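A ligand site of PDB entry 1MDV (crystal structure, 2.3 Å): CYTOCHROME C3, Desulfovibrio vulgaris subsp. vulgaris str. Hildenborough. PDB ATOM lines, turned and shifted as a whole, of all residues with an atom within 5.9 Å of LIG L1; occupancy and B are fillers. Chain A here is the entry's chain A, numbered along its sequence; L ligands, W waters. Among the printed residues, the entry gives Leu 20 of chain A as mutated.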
ATOM      1  N   LEU A   9      33.318  10.564  22.709  1.00  0.00           N
ATOM      2  CA  LEU A   9      34.585  11.251  22.441  1.00  0.00           C
ATOM      3  C   LEU A   9      35.247  11.918  23.656  1.00  0.00           C
ATOM      4  O   LEU A   9      34.612  12.138  24.690  1.00  0.00           O
ATOM      5  CB  LEU A   9      34.401  12.333  21.362  1.00  0.00           C
ATOM      6  CG  LEU A   9      33.932  11.986  19.951  1.00  0.00           C
ATOM      7  CD1 LEU A   9      32.434  11.659  19.940  1.00  0.00           C
ATOM      8  CD2 LEU A   9      34.225  13.171  19.033  1.00  0.00           C
ATOM      9  N   LYS A  10      36.529  12.247  23.497  1.00  0.00           N
ATOM     10  CA  LYS A  10      37.307  12.931  24.530  1.00  0.00           C
ATOM     11  C   LYS A  10      37.804  14.259  23.950  1.00  0.00           C
ATOM     12  O   LYS A  10      38.581  14.276  22.983  1.00  0.00           O
ATOM     13  CB  LYS A  10      38.510  12.074  24.990  1.00  0.00           C
ATOM     14  CG  LYS A  10      39.467  12.808  25.938  1.00  0.00           C
ATOM     15  CD  LYS A  10      40.536  11.883  26.515  1.00  0.00           C
ATOM     16  CE  LYS A  10      40.120  11.270  27.852  1.00  0.00           C
ATOM     17  NZ  LYS A  10      38.865  10.448  27.807  1.00  0.00           N
ATOM     18  N   MET A  11      37.308  15.358  24.520  1.00  0.00           N
ATOM     19  CA  MET A  11      37.680  16.703  24.073  1.00  0.00           C
ATOM     20  C   MET A  11      39.136  16.996  24.483  1.00  0.00           C
ATOM     21  O   MET A  11      39.394  17.649  25.501  1.00  0.00           O
ATOM     22  CB  MET A  11      36.725  17.760  24.648  1.00  0.00           C
ATOM     23  CG  MET A  11      35.216  17.483  24.429  1.00  0.00           C
ATOM     24  SD  MET A  11      34.388  16.482  25.724  1.00  0.00           S
ATOM     25  CE  MET A  11      32.963  17.519  26.133  1.00  0.00           C
ATOM     26  N   LEU A  20      32.343  12.626  26.394  1.00  0.00           N
ATOM     27  CA  LEU A  20      30.886  12.669  26.183  1.00  0.00           C
ATOM     28  C   LEU A  20      30.413  11.464  25.382  1.00  0.00           C
ATOM     29  O   LEU A  20      30.613  11.396  24.169  1.00  0.00           O
ATOM     30  CB  LEU A  20      30.413  13.942  25.476  1.00  0.00           C
ATOM     31  CG  LEU A  20      28.874  13.894  25.372  1.00  0.00           C
ATOM     32  CD1 LEU A  20      28.225  15.038  26.120  1.00  0.00           C
ATOM     33  CD2 LEU A  20      28.413  13.884  23.938  1.00  0.00           C
ATOM     34  N   HIS A  22      27.831   9.430  23.460  1.00  0.00           N
ATOM     35  CA  HIS A  22      26.583   9.657  22.727  1.00  0.00           C
ATOM     36  C   HIS A  22      25.563   8.543  23.014  1.00  0.00           C
ATOM     37  O   HIS A  22      24.365   8.730  22.777  1.00  0.00           O
ATOM     38  CB  HIS A  22      26.822   9.773  21.213  1.00  0.00           C
ATOM     39  CG  HIS A  22      27.191  11.146  20.743  1.00  0.00           C
ATOM     40  ND1 HIS A  22      28.474  11.544  20.449  1.00  0.00           N
ATOM     41  CD2 HIS A  22      26.401  12.223  20.466  1.00  0.00           C
ATOM     42  CE1 HIS A  22      28.432  12.822  20.002  1.00  0.00           C
ATOM     43  NE2 HIS A  22      27.195  13.285  19.989  1.00  0.00           N
ATOM     44  N   HIS A  25      23.365   9.376  26.127  1.00  0.00           N
ATOM     45  CA  HIS A  25      22.498  10.537  25.910  1.00  0.00           C
ATOM     46  C   HIS A  25      21.484  10.369  24.745  1.00  0.00           C
ATOM     47  O   HIS A  25      20.975  11.361  24.217  1.00  0.00           O
ATOM     48  CB  HIS A  25      23.351  11.803  25.682  1.00  0.00           C
ATOM     49  CG  HIS A  25      24.073  12.288  26.906  1.00  0.00           C
ATOM     50  ND1 HIS A  25      25.355  11.943  27.229  1.00  0.00           N
ATOM     51  CD2 HIS A  25      23.665  13.127  27.887  1.00  0.00           C
ATOM     52  CE1 HIS A  25      25.701  12.566  28.359  1.00  0.00           C
ATOM     53  NE2 HIS A  25      24.706  13.313  28.811  1.00  0.00           N
ATOM     54  N   VAL A  28      17.995  12.425  24.268  1.00  0.00           N
ATOM     55  CA  VAL A  28      18.051  13.874  24.022  1.00  0.00           C
ATOM     56  C   VAL A  28      18.204  14.128  22.510  1.00  0.00           C
ATOM     57  O   VAL A  28      18.981  13.463  21.838  1.00  0.00           O
ATOM     58  CB  VAL A  28      19.277  14.523  24.752  1.00  0.00           C
ATOM     59  CG1 VAL A  28      19.330  16.033  24.479  1.00  0.00           C
ATOM     60  CG2 VAL A  28      19.226  14.261  26.254  1.00  0.00           C
ATOM     61  N   LYS A  29      17.465  15.111  21.991  1.00  0.00           N
ATOM     62  CA  LYS A  29      17.524  15.458  20.570  1.00  0.00           C
ATOM     63  C   LYS A  29      18.887  16.095  20.266  1.00  0.00           C
ATOM     64  O   LYS A  29      19.389  16.878  21.082  1.00  0.00           O
ATOM     65  CB  LYS A  29      16.390  16.432  20.215  1.00  0.00           C
ATOM     66  CG  LYS A  29      14.996  15.891  20.506  1.00  0.00           C
ATOM     67  CD  LYS A  29      13.920  16.942  20.243  1.00  0.00           C
ATOM     68  CE  LYS A  29      12.534  16.402  20.593  1.00  0.00           C
ATOM     69  NZ  LYS A  29      11.449  17.399  20.361  1.00  0.00           N
ATOM     70  N   CYS A  30      19.479  15.758  19.125  1.00  0.00           N
ATOM     71  CA  CYS A  30      20.788  16.301  18.746  1.00  0.00           C
ATOM     72  C   CYS A  30      20.808  17.826  18.805  1.00  0.00           C
ATOM     73  O   CYS A  30      21.807  18.435  19.200  1.00  0.00           O
ATOM     74  CB  CYS A  30      21.180  15.875  17.314  1.00  0.00           C
ATOM     75  SG  CYS A  30      20.695  14.206  16.739  1.00  0.00           S
ATOM     76  N   GLY A  31      19.677  18.439  18.427  1.00  0.00           N
ATOM     77  CA  GLY A  31      19.552  19.881  18.400  1.00  0.00           C
ATOM     78  C   GLY A  31      19.658  20.620  19.714  1.00  0.00           C
ATOM     79  O   GLY A  31      19.983  21.814  19.724  1.00  0.00           O
ATOM     80  N   ASP A  32      19.357  19.945  20.818  1.00  0.00           N
ATOM     81  CA  ASP A  32      19.436  20.581  22.135  1.00  0.00           C
ATOM     82  C   ASP A  32      20.879  20.963  22.434  1.00  0.00           C
ATOM     83  O   ASP A  32      21.154  22.038  22.963  1.00  0.00           O
ATOM     84  CB  ASP A  32      18.892  19.651  23.219  1.00  0.00           C
ATOM     85  CG  ASP A  32      17.386  19.436  23.097  1.00  0.00           C
ATOM     86  OD1 ASP A  32      16.744  20.114  22.279  1.00  0.00           O
ATOM     87  OD2 ASP A  32      16.849  18.576  23.838  1.00  0.00           O
ATOM     88  N   CYS A  33      21.817  20.087  22.053  1.00  0.00           N
ATOM     89  CA  CYS A  33      23.230  20.349  22.262  1.00  0.00           C
ATOM     90  C   CYS A  33      23.805  21.025  21.037  1.00  0.00           C
ATOM     91  O   CYS A  33      24.379  22.110  21.145  1.00  0.00           O
ATOM     92  CB  CYS A  33      23.973  19.054  22.582  1.00  0.00           C
ATOM     93  SG  CYS A  33      23.376  18.284  24.120  1.00  0.00           S
ATOM     94  N   HIS A  34      23.674  20.400  19.875  1.00  0.00           N
ATOM     95  CA  HIS A  34      24.164  20.996  18.625  1.00  0.00           C
ATOM     96  C   HIS A  34      23.080  21.979  18.171  1.00  0.00           C
ATOM     97  O   HIS A  34      22.341  21.711  17.223  1.00  0.00           O
ATOM     98  CB  HIS A  34      24.386  19.899  17.578  1.00  0.00           C
ATOM     99  CG  HIS A  34      25.388  18.857  17.985  1.00  0.00           C
ATOM    100  ND1 HIS A  34      26.751  19.015  17.918  1.00  0.00           N
ATOM    101  CD2 HIS A  34      25.200  17.596  18.467  1.00  0.00           C
ATOM    102  CE1 HIS A  34      27.329  17.884  18.354  1.00  0.00           C
ATOM    103  NE2 HIS A  34      26.437  16.989  18.699  1.00  0.00           N
ATOM    104  N   TYR A  43      27.411  21.124  13.309  1.00  0.00           N
ATOM    105  CA  TYR A  43      27.946  19.944  13.985  1.00  0.00           C
ATOM    106  C   TYR A  43      29.440  20.005  14.238  1.00  0.00           C
ATOM    107  O   TYR A  43      30.104  18.974  14.344  1.00  0.00           O
ATOM    108  CB  TYR A  43      27.585  18.665  13.224  1.00  0.00           C
ATOM    109  CG  TYR A  43      26.146  18.262  13.403  1.00  0.00           C
ATOM    110  CD1 TYR A  43      25.161  18.745  12.549  1.00  0.00           C
ATOM    111  CD2 TYR A  43      25.771  17.432  14.461  1.00  0.00           C
ATOM    112  CE1 TYR A  43      23.818  18.415  12.748  1.00  0.00           C
ATOM    113  CE2 TYR A  43      24.440  17.096  14.654  1.00  0.00           C
ATOM    114  CZ  TYR A  43      23.463  17.594  13.801  1.00  0.00           C
ATOM    115  OH  TYR A  43      22.149  17.267  14.005  1.00  0.00           O
ATOM    116  N   ARG A  44      29.973  21.217  14.351  1.00  0.00           N
ATOM    117  CA  ARG A  44      31.393  21.401  14.617  1.00  0.00           C
ATOM    118  C   ARG A  44      31.682  21.429  16.126  1.00  0.00           C
ATOM    119  O   ARG A  44      30.751  21.557  16.931  1.00  0.00           O
ATOM    120  CB  ARG A  44      31.889  22.693  13.953  1.00  0.00           C
ATOM    121  CG  ARG A  44      31.833  22.652  12.431  1.00  0.00           C
ATOM    122  CD  ARG A  44      32.358  23.941  11.801  1.00  0.00           C
ATOM    123  NE  ARG A  44      31.413  25.056  11.947  1.00  0.00           N
ATOM    124  CZ  ARG A  44      31.657  26.304  11.563  1.00  0.00           C
ATOM    125  NH1 ARG A  44      32.821  26.621  11.000  1.00  0.00           N
ATOM    126  NH2 ARG A  44      30.732  27.230  11.734  1.00  0.00           N
ATOM    127  N   LYS A  45      32.947  21.295  16.488  1.00  0.00           N
ATOM    128  CA  LYS A  45      33.360  21.299  17.891  1.00  0.00           C
ATOM    129  C   LYS A  45      32.902  22.592  18.563  1.00  0.00           C
ATOM    130  O   LYS A  45      32.874  23.644  17.933  1.00  0.00           O
ATOM    131  CB  LYS A  45      34.874  21.136  18.020  1.00  0.00           C
ATOM    132  CG  LYS A  45      35.411  19.824  17.473  1.00  0.00           C
ATOM    133  CD  LYS A  45      36.898  19.680  17.726  1.00  0.00           C
ATOM    134  CE  LYS A  45      37.210  19.513  19.210  1.00  0.00           C
ATOM    135  NZ  LYS A  45      38.670  19.414  19.482  1.00  0.00           N
ATOM    136  N   CYS A  46      32.530  22.507  19.841  1.00  0.00           N
ATOM    137  CA  CYS A  46      32.049  23.666  20.590  1.00  0.00           C
ATOM    138  C   CYS A  46      33.087  24.776  20.776  1.00  0.00           C
ATOM    139  O   CYS A  46      32.729  25.946  20.883  1.00  0.00           O
ATOM    140  CB  CYS A  46      31.501  23.253  21.967  1.00  0.00           C
ATOM    141  SG  CYS A  46      30.446  21.758  22.023  1.00  0.00           S
ATOM    142  N   GLY A  47      34.364  24.422  20.788  1.00  0.00           N
ATOM    143  CA  GLY A  47      35.413  25.415  20.984  1.00  0.00           C
ATOM    144  C   GLY A  47      36.244  25.849  19.788  1.00  0.00           C
ATOM    145  O   GLY A  47      37.463  26.001  19.904  1.00  0.00           O
HETATM  146  C1  LIG L   1      30.264  15.591  18.960  1.00  0.00           C
HETATM  147  C2  LIG L   1      26.551  14.507  16.045  1.00  0.00           C
HETATM  148  C3  LIG L   1      23.727  14.284  19.932  1.00  0.00           C
HETATM  149  C4  LIG L   1      27.059  16.755  22.359  1.00  0.00           C
HETATM  150  C5  LIG L   1      29.527  15.183  17.836  1.00  0.00           C
HETATM  151  C6  LIG L   1      30.069  14.982  16.509  1.00  0.00           C
HETATM  152  C7  LIG L   1      29.033  14.811  15.664  1.00  0.00           C
HETATM  153  C8  LIG L   1      27.826  14.797  16.493  1.00  0.00           C
HETATM  154  C9  LIG L   1      29.129  14.722  14.145  1.00  0.00           C
HETATM  155  C10 LIG L   1      31.536  14.831  16.167  1.00  0.00           C
HETATM  156  C11 LIG L   1      32.244  16.141  15.944  1.00  0.00           C
HETATM  157  C12 LIG L   1      33.748  15.984  15.862  1.00  0.00           C
HETATM  158  O1  LIG L   1      34.436  16.238  16.873  1.00  0.00           O
HETATM  159  O2  LIG L   1      34.248  15.589  14.780  1.00  0.00           O
HETATM  160  C13 LIG L   1      25.415  14.443  16.839  1.00  0.00           C
HETATM  161  C14 LIG L   1      24.132  13.935  16.384  1.00  0.00           C
HETATM  162  C15 LIG L   1      23.375  13.733  17.476  1.00  0.00           C
HETATM  163  C16 LIG L   1      24.179  14.189  18.625  1.00  0.00           C
HETATM  164  C17 LIG L   1      23.706  13.684  14.953  1.00  0.00           C
HETATM  165  C18 LIG L   1      21.949  13.162  17.547  1.00  0.00           C
HETATM  166  C19 LIG L   1      21.721  11.668  17.274  1.00  0.00           C
HETATM  167  C20 LIG L   1      24.398  14.926  20.963  1.00  0.00           C
HETATM  168  C21 LIG L   1      23.750  15.375  22.201  1.00  0.00           C
HETATM  169  C22 LIG L   1      24.681  16.130  22.876  1.00  0.00           C
HETATM  170  C23 LIG L   1      25.875  16.126  22.039  1.00  0.00           C
HETATM  171  C24 LIG L   1      22.273  15.171  22.539  1.00  0.00           C
HETATM  172  C25 LIG L   1      24.508  16.841  24.227  1.00  0.00           C
HETATM  173  C26 LIG L   1      24.201  15.957  25.445  1.00  0.00           C
HETATM  174  C27 LIG L   1      28.230  16.721  21.614  1.00  0.00           C
HETATM  175  C28 LIG L   1      29.529  17.154  22.106  1.00  0.00           C
HETATM  176  C29 LIG L   1      30.433  16.683  21.213  1.00  0.00           C
HETATM  177  C30 LIG L   1      29.715  16.015  20.161  1.00  0.00           C
HETATM  178  C31 LIG L   1      29.840  17.902  23.416  1.00  0.00           C
HETATM  179  C32 LIG L   1      31.938  16.747  21.382  1.00  0.00           C
HETATM  180  C33 LIG L   1      32.581  17.834  20.543  1.00  0.00           C
HETATM  181  C34 LIG L   1      34.045  18.052  20.880  1.00  0.00           C
HETATM  182  O3  LIG L   1      34.821  17.070  20.880  1.00  0.00           O
HETATM  183  O4  LIG L   1      34.425  19.211  21.127  1.00  0.00           O
HETATM  184  N1  LIG L   1      28.147  15.048  17.825  1.00  0.00           N
HETATM  185  N2  LIG L   1      25.430  14.620  18.221  1.00  0.00           N
HETATM  186  N3  LIG L   1      25.678  15.411  20.871  1.00  0.00           N
HETATM  187  N4  LIG L   1      28.362  16.015  20.413  1.00  0.00           N
HETATM  188 FE1  LIG L   1      26.934  15.169  19.357  1.00  0.00          FE
HETATM  189  C1  LG2 L   2      24.500  11.237  31.988  1.00  0.00           C
HETATM  190  C2  LG2 L   2      28.204  14.107  30.727  1.00  0.00           C
HETATM  191  C3  LG2 L   2      25.102  17.286  28.957  1.00  0.00           C
HETATM  192  C4  LG2 L   2      21.404  14.542  30.283  1.00  0.00           C
HETATM  193  C5  LG2 L   2      25.765  11.815  31.887  1.00  0.00           C
HETATM  194  C6  LG2 L   2      26.990  11.227  32.411  1.00  0.00           C
HETATM  195  C7  LG2 L   2      28.012  11.962  32.008  1.00  0.00           C
HETATM  196  C8  LG2 L   2      27.446  13.101  31.307  1.00  0.00           C
HETATM  197  C9  LG2 L   2      29.474  11.641  32.283  1.00  0.00           C
HETATM  198  C10 LG2 L   2      27.114  10.074  33.383  1.00  0.00           C
HETATM  199  C11 LG2 L   2      27.022   8.762  32.646  1.00  0.00           C
HETATM  200  C12 LG2 L   2      27.620   7.605  33.412  1.00  0.00           C
HETATM  201  O1  LG2 L   2      27.293   7.427  34.604  1.00  0.00           O
HETATM  202  O2  LG2 L   2      28.443   6.862  32.812  1.00  0.00           O
HETATM  203  C13 LG2 L   2      27.694  15.245  30.131  1.00  0.00           C
HETATM  204  C14 LG2 L   2      28.501  16.348  29.588  1.00  0.00           C
HETATM  205  C15 LG2 L   2      27.624  17.298  29.146  1.00  0.00           C
HETATM  206  C16 LG2 L   2      26.267  16.699  29.391  1.00  0.00           C
HETATM  207  C17 LG2 L   2      30.024  16.384  29.466  1.00  0.00           C
HETATM  208  C18 LG2 L   2      27.910  18.689  28.479  1.00  0.00           C
HETATM  209  C19 LG2 L   2      28.795  18.657  27.226  1.00  0.00           C
HETATM  210  C20 LG2 L   2      23.847  16.822  29.240  1.00  0.00           C
HETATM  211  C21 LG2 L   2      22.650  17.618  28.944  1.00  0.00           C
HETATM  212  C22 LG2 L   2      21.609  16.886  29.357  1.00  0.00           C
HETATM  213  C23 LG2 L   2      22.164  15.633  29.877  1.00  0.00           C
HETATM  214  C24 LG2 L   2      22.603  19.027  28.349  1.00  0.00           C
HETATM  215  C25 LG2 L   2      20.113  17.285  29.309  1.00  0.00           C
HETATM  216  C26 LG2 L   2      19.530  18.066  28.126  1.00  0.00           C
HETATM  217  C27 LG2 L   2      21.914  13.347  30.804  1.00  0.00           C
HETATM  218  C28 LG2 L   2      21.128  12.197  31.202  1.00  0.00           C
HETATM  219  C29 LG2 L   2      21.987  11.305  31.781  1.00  0.00           C
HETATM  220  C30 LG2 L   2      23.326  11.884  31.671  1.00  0.00           C
HETATM  221  C31 LG2 L   2      19.636  11.945  30.948  1.00  0.00           C
HETATM  222  C32 LG2 L   2      21.611   9.958  32.370  1.00  0.00           C
HETATM  223  C33 LG2 L   2      21.382   9.935  33.873  1.00  0.00           C
HETATM  224  C34 LG2 L   2      20.990   8.554  34.361  1.00  0.00           C
HETATM  225  O3  LG2 L   2      21.727   7.586  34.086  1.00  0.00           O
HETATM  226  O4  LG2 L   2      19.930   8.427  35.023  1.00  0.00           O
HETATM  227  N1  LG2 L   2      26.045  13.030  31.267  1.00  0.00           N
HETATM  228  N2  LG2 L   2      26.324  15.468  30.010  1.00  0.00           N
HETATM  229  N3  LG2 L   2      23.551  15.634  29.869  1.00  0.00           N
HETATM  230  N4  LG2 L   2      23.270  13.128  31.059  1.00  0.00           N
HETATM  231 FE1  LG2 L   2      24.749  14.322  30.585  1.00  0.00          FE
HETATM  232  C1  LG3 L   3      25.140  30.143  22.687  1.00  0.00           C
HETATM  233  C2  LG3 L   3      26.476  25.672  24.026  1.00  0.00           C
HETATM  234  C3  LG3 L   3      28.553  25.068  19.712  1.00  0.00           C
HETATM  235  C4  LG3 L   3      27.982  29.768  18.803  1.00  0.00           C
HETATM  236  C5  LG3 L   3      25.296  28.967  23.422  1.00  0.00           C
HETATM  237  C6  LG3 L   3      24.828  28.774  24.798  1.00  0.00           C
HETATM  238  C7  LG3 L   3      25.172  27.514  25.148  1.00  0.00           C
HETATM  239  C8  LG3 L   3      25.904  26.945  24.028  1.00  0.00           C
HETATM  240  C9  LG3 L   3      24.800  26.839  26.462  1.00  0.00           C
HETATM  241  C10 LG3 L   3      24.154  29.788  25.723  1.00  0.00           C
HETATM  242  C11 LG3 L   3      24.992  31.008  26.073  1.00  0.00           C
HETATM  243  C12 LG3 L   3      24.270  32.016  26.968  1.00  0.00           C
HETATM  244  O1  LG3 L   3      23.023  31.945  27.086  1.00  0.00           O
HETATM  245  O2  LG3 L   3      24.939  32.887  27.549  1.00  0.00           O
HETATM  246  C13 LG3 L   3      27.187  25.105  22.981  1.00  0.00           C
HETATM  247  C14 LG3 L   3      27.759  23.741  22.971  1.00  0.00           C
HETATM  248  C15 LG3 L   3      28.275  23.539  21.711  1.00  0.00           C
HETATM  249  C16 LG3 L   3      28.054  24.796  20.980  1.00  0.00           C
HETATM  250  C17 LG3 L   3      27.850  22.764  24.148  1.00  0.00           C
HETATM  251  C18 LG3 L   3      28.947  22.287  21.127  1.00  0.00           C
HETATM  252  C19 LG3 L   3      28.010  21.105  20.887  1.00  0.00           C
HETATM  253  C20 LG3 L   3      28.501  26.279  19.023  1.00  0.00           C
HETATM  254  C21 LG3 L   3      29.248  26.555  17.801  1.00  0.00           C
HETATM  255  C22 LG3 L   3      29.230  27.911  17.620  1.00  0.00           C
HETATM  256  C23 LG3 L   3      28.372  28.431  18.677  1.00  0.00           C
HETATM  257  C24 LG3 L   3      29.903  25.524  16.896  1.00  0.00           C
HETATM  258  C25 LG3 L   3      29.959  28.730  16.536  1.00  0.00           C
HETATM  259  C26 LG3 L   3      29.294  28.663  15.155  1.00  0.00           C
HETATM  260  C27 LG3 L   3      27.096  30.267  19.748  1.00  0.00           C
HETATM  261  C28 LG3 L   3      26.463  31.567  19.687  1.00  0.00           C
HETATM  262  C29 LG3 L   3      25.584  31.642  20.700  1.00  0.00           C
HETATM  263  C30 LG3 L   3      25.721  30.404  21.450  1.00  0.00           C
HETATM  264  C31 LG3 L   3      26.700  32.634  18.629  1.00  0.00           C
HETATM  265  C32 LG3 L   3      24.578  32.774  20.927  1.00  0.00           C
HETATM  266  C33 LG3 L   3      23.352  32.713  20.010  1.00  0.00           C
HETATM  267  C34 LG3 L   3      22.325  33.802  20.309  1.00  0.00           C
HETATM  268  O3  LG3 L   3      22.711  34.981  20.389  1.00  0.00           O
HETATM  269  O4  LG3 L   3      21.128  33.467  20.456  1.00  0.00           O
HETATM  270  N1  LG3 L   3      25.986  27.846  22.969  1.00  0.00           N
HETATM  271  N2  LG3 L   3      27.417  25.749  21.759  1.00  0.00           N
HETATM  272  N3  LG3 L   3      27.967  27.432  19.554  1.00  0.00           N
HETATM  273  N4  LG3 L   3      26.601  29.534  20.798  1.00  0.00           N
HETATM  274 FE1  LG3 L   3      26.958  27.630  21.226  1.00  0.00          FE
HETATM  275  O   HOH W   1      23.647  11.277  21.650  1.00  0.00           O
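The backbone NH of Leu 20 sits at hydrogen-bond distance from the backbone carbonyl oxygen of Leu 9, 2.9 Å away.
The side-chain sulfur of Cys 30 is bonded to a carbon (C18) of LIG L1 (1.8 Å). C25 of LIG L1 is covalently linked to SG of Cys 33 (1.8 Å). FE1 of LIG L1 is bound by NE2 of His 34, 2.0 Å away. NE2 of His 22 binds FE1 of LIG L1 (2.0 Å). NE2 of His 25 is bound to FE1 of LG2 L2 (2.0 Å). The side-chain sulfur of Cys 46 is covalently linked to a carbon (C18) of LG3 L3, at 1.8 Å.
Leu 9 touches LIG L1 (CD2 to O1, 3.8 Å). CG of Met 11 touches O3 of LIG L1 (3.6 Å). Leu 20 touches LIG L1. His 25 touches LIG L1 (CD2 to C26, 3.8 Å). CG1 of Val 28 touches C24 of LIG L1, 3.6 Å away. O of Lys 29 touches C24 of LIG L1 (3.7 Å). Tyr 43 touches LIG L1. Lys 45 touches LIG L1. Hydrophobic or aromatic side chains that line LIG L1: Leu 9, Met 11, Leu 20, His 22, His 25, Val 28, His 34 and Tyr 43. Of the 18 residues printed, 12 come within 4 Å of LIG L1.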
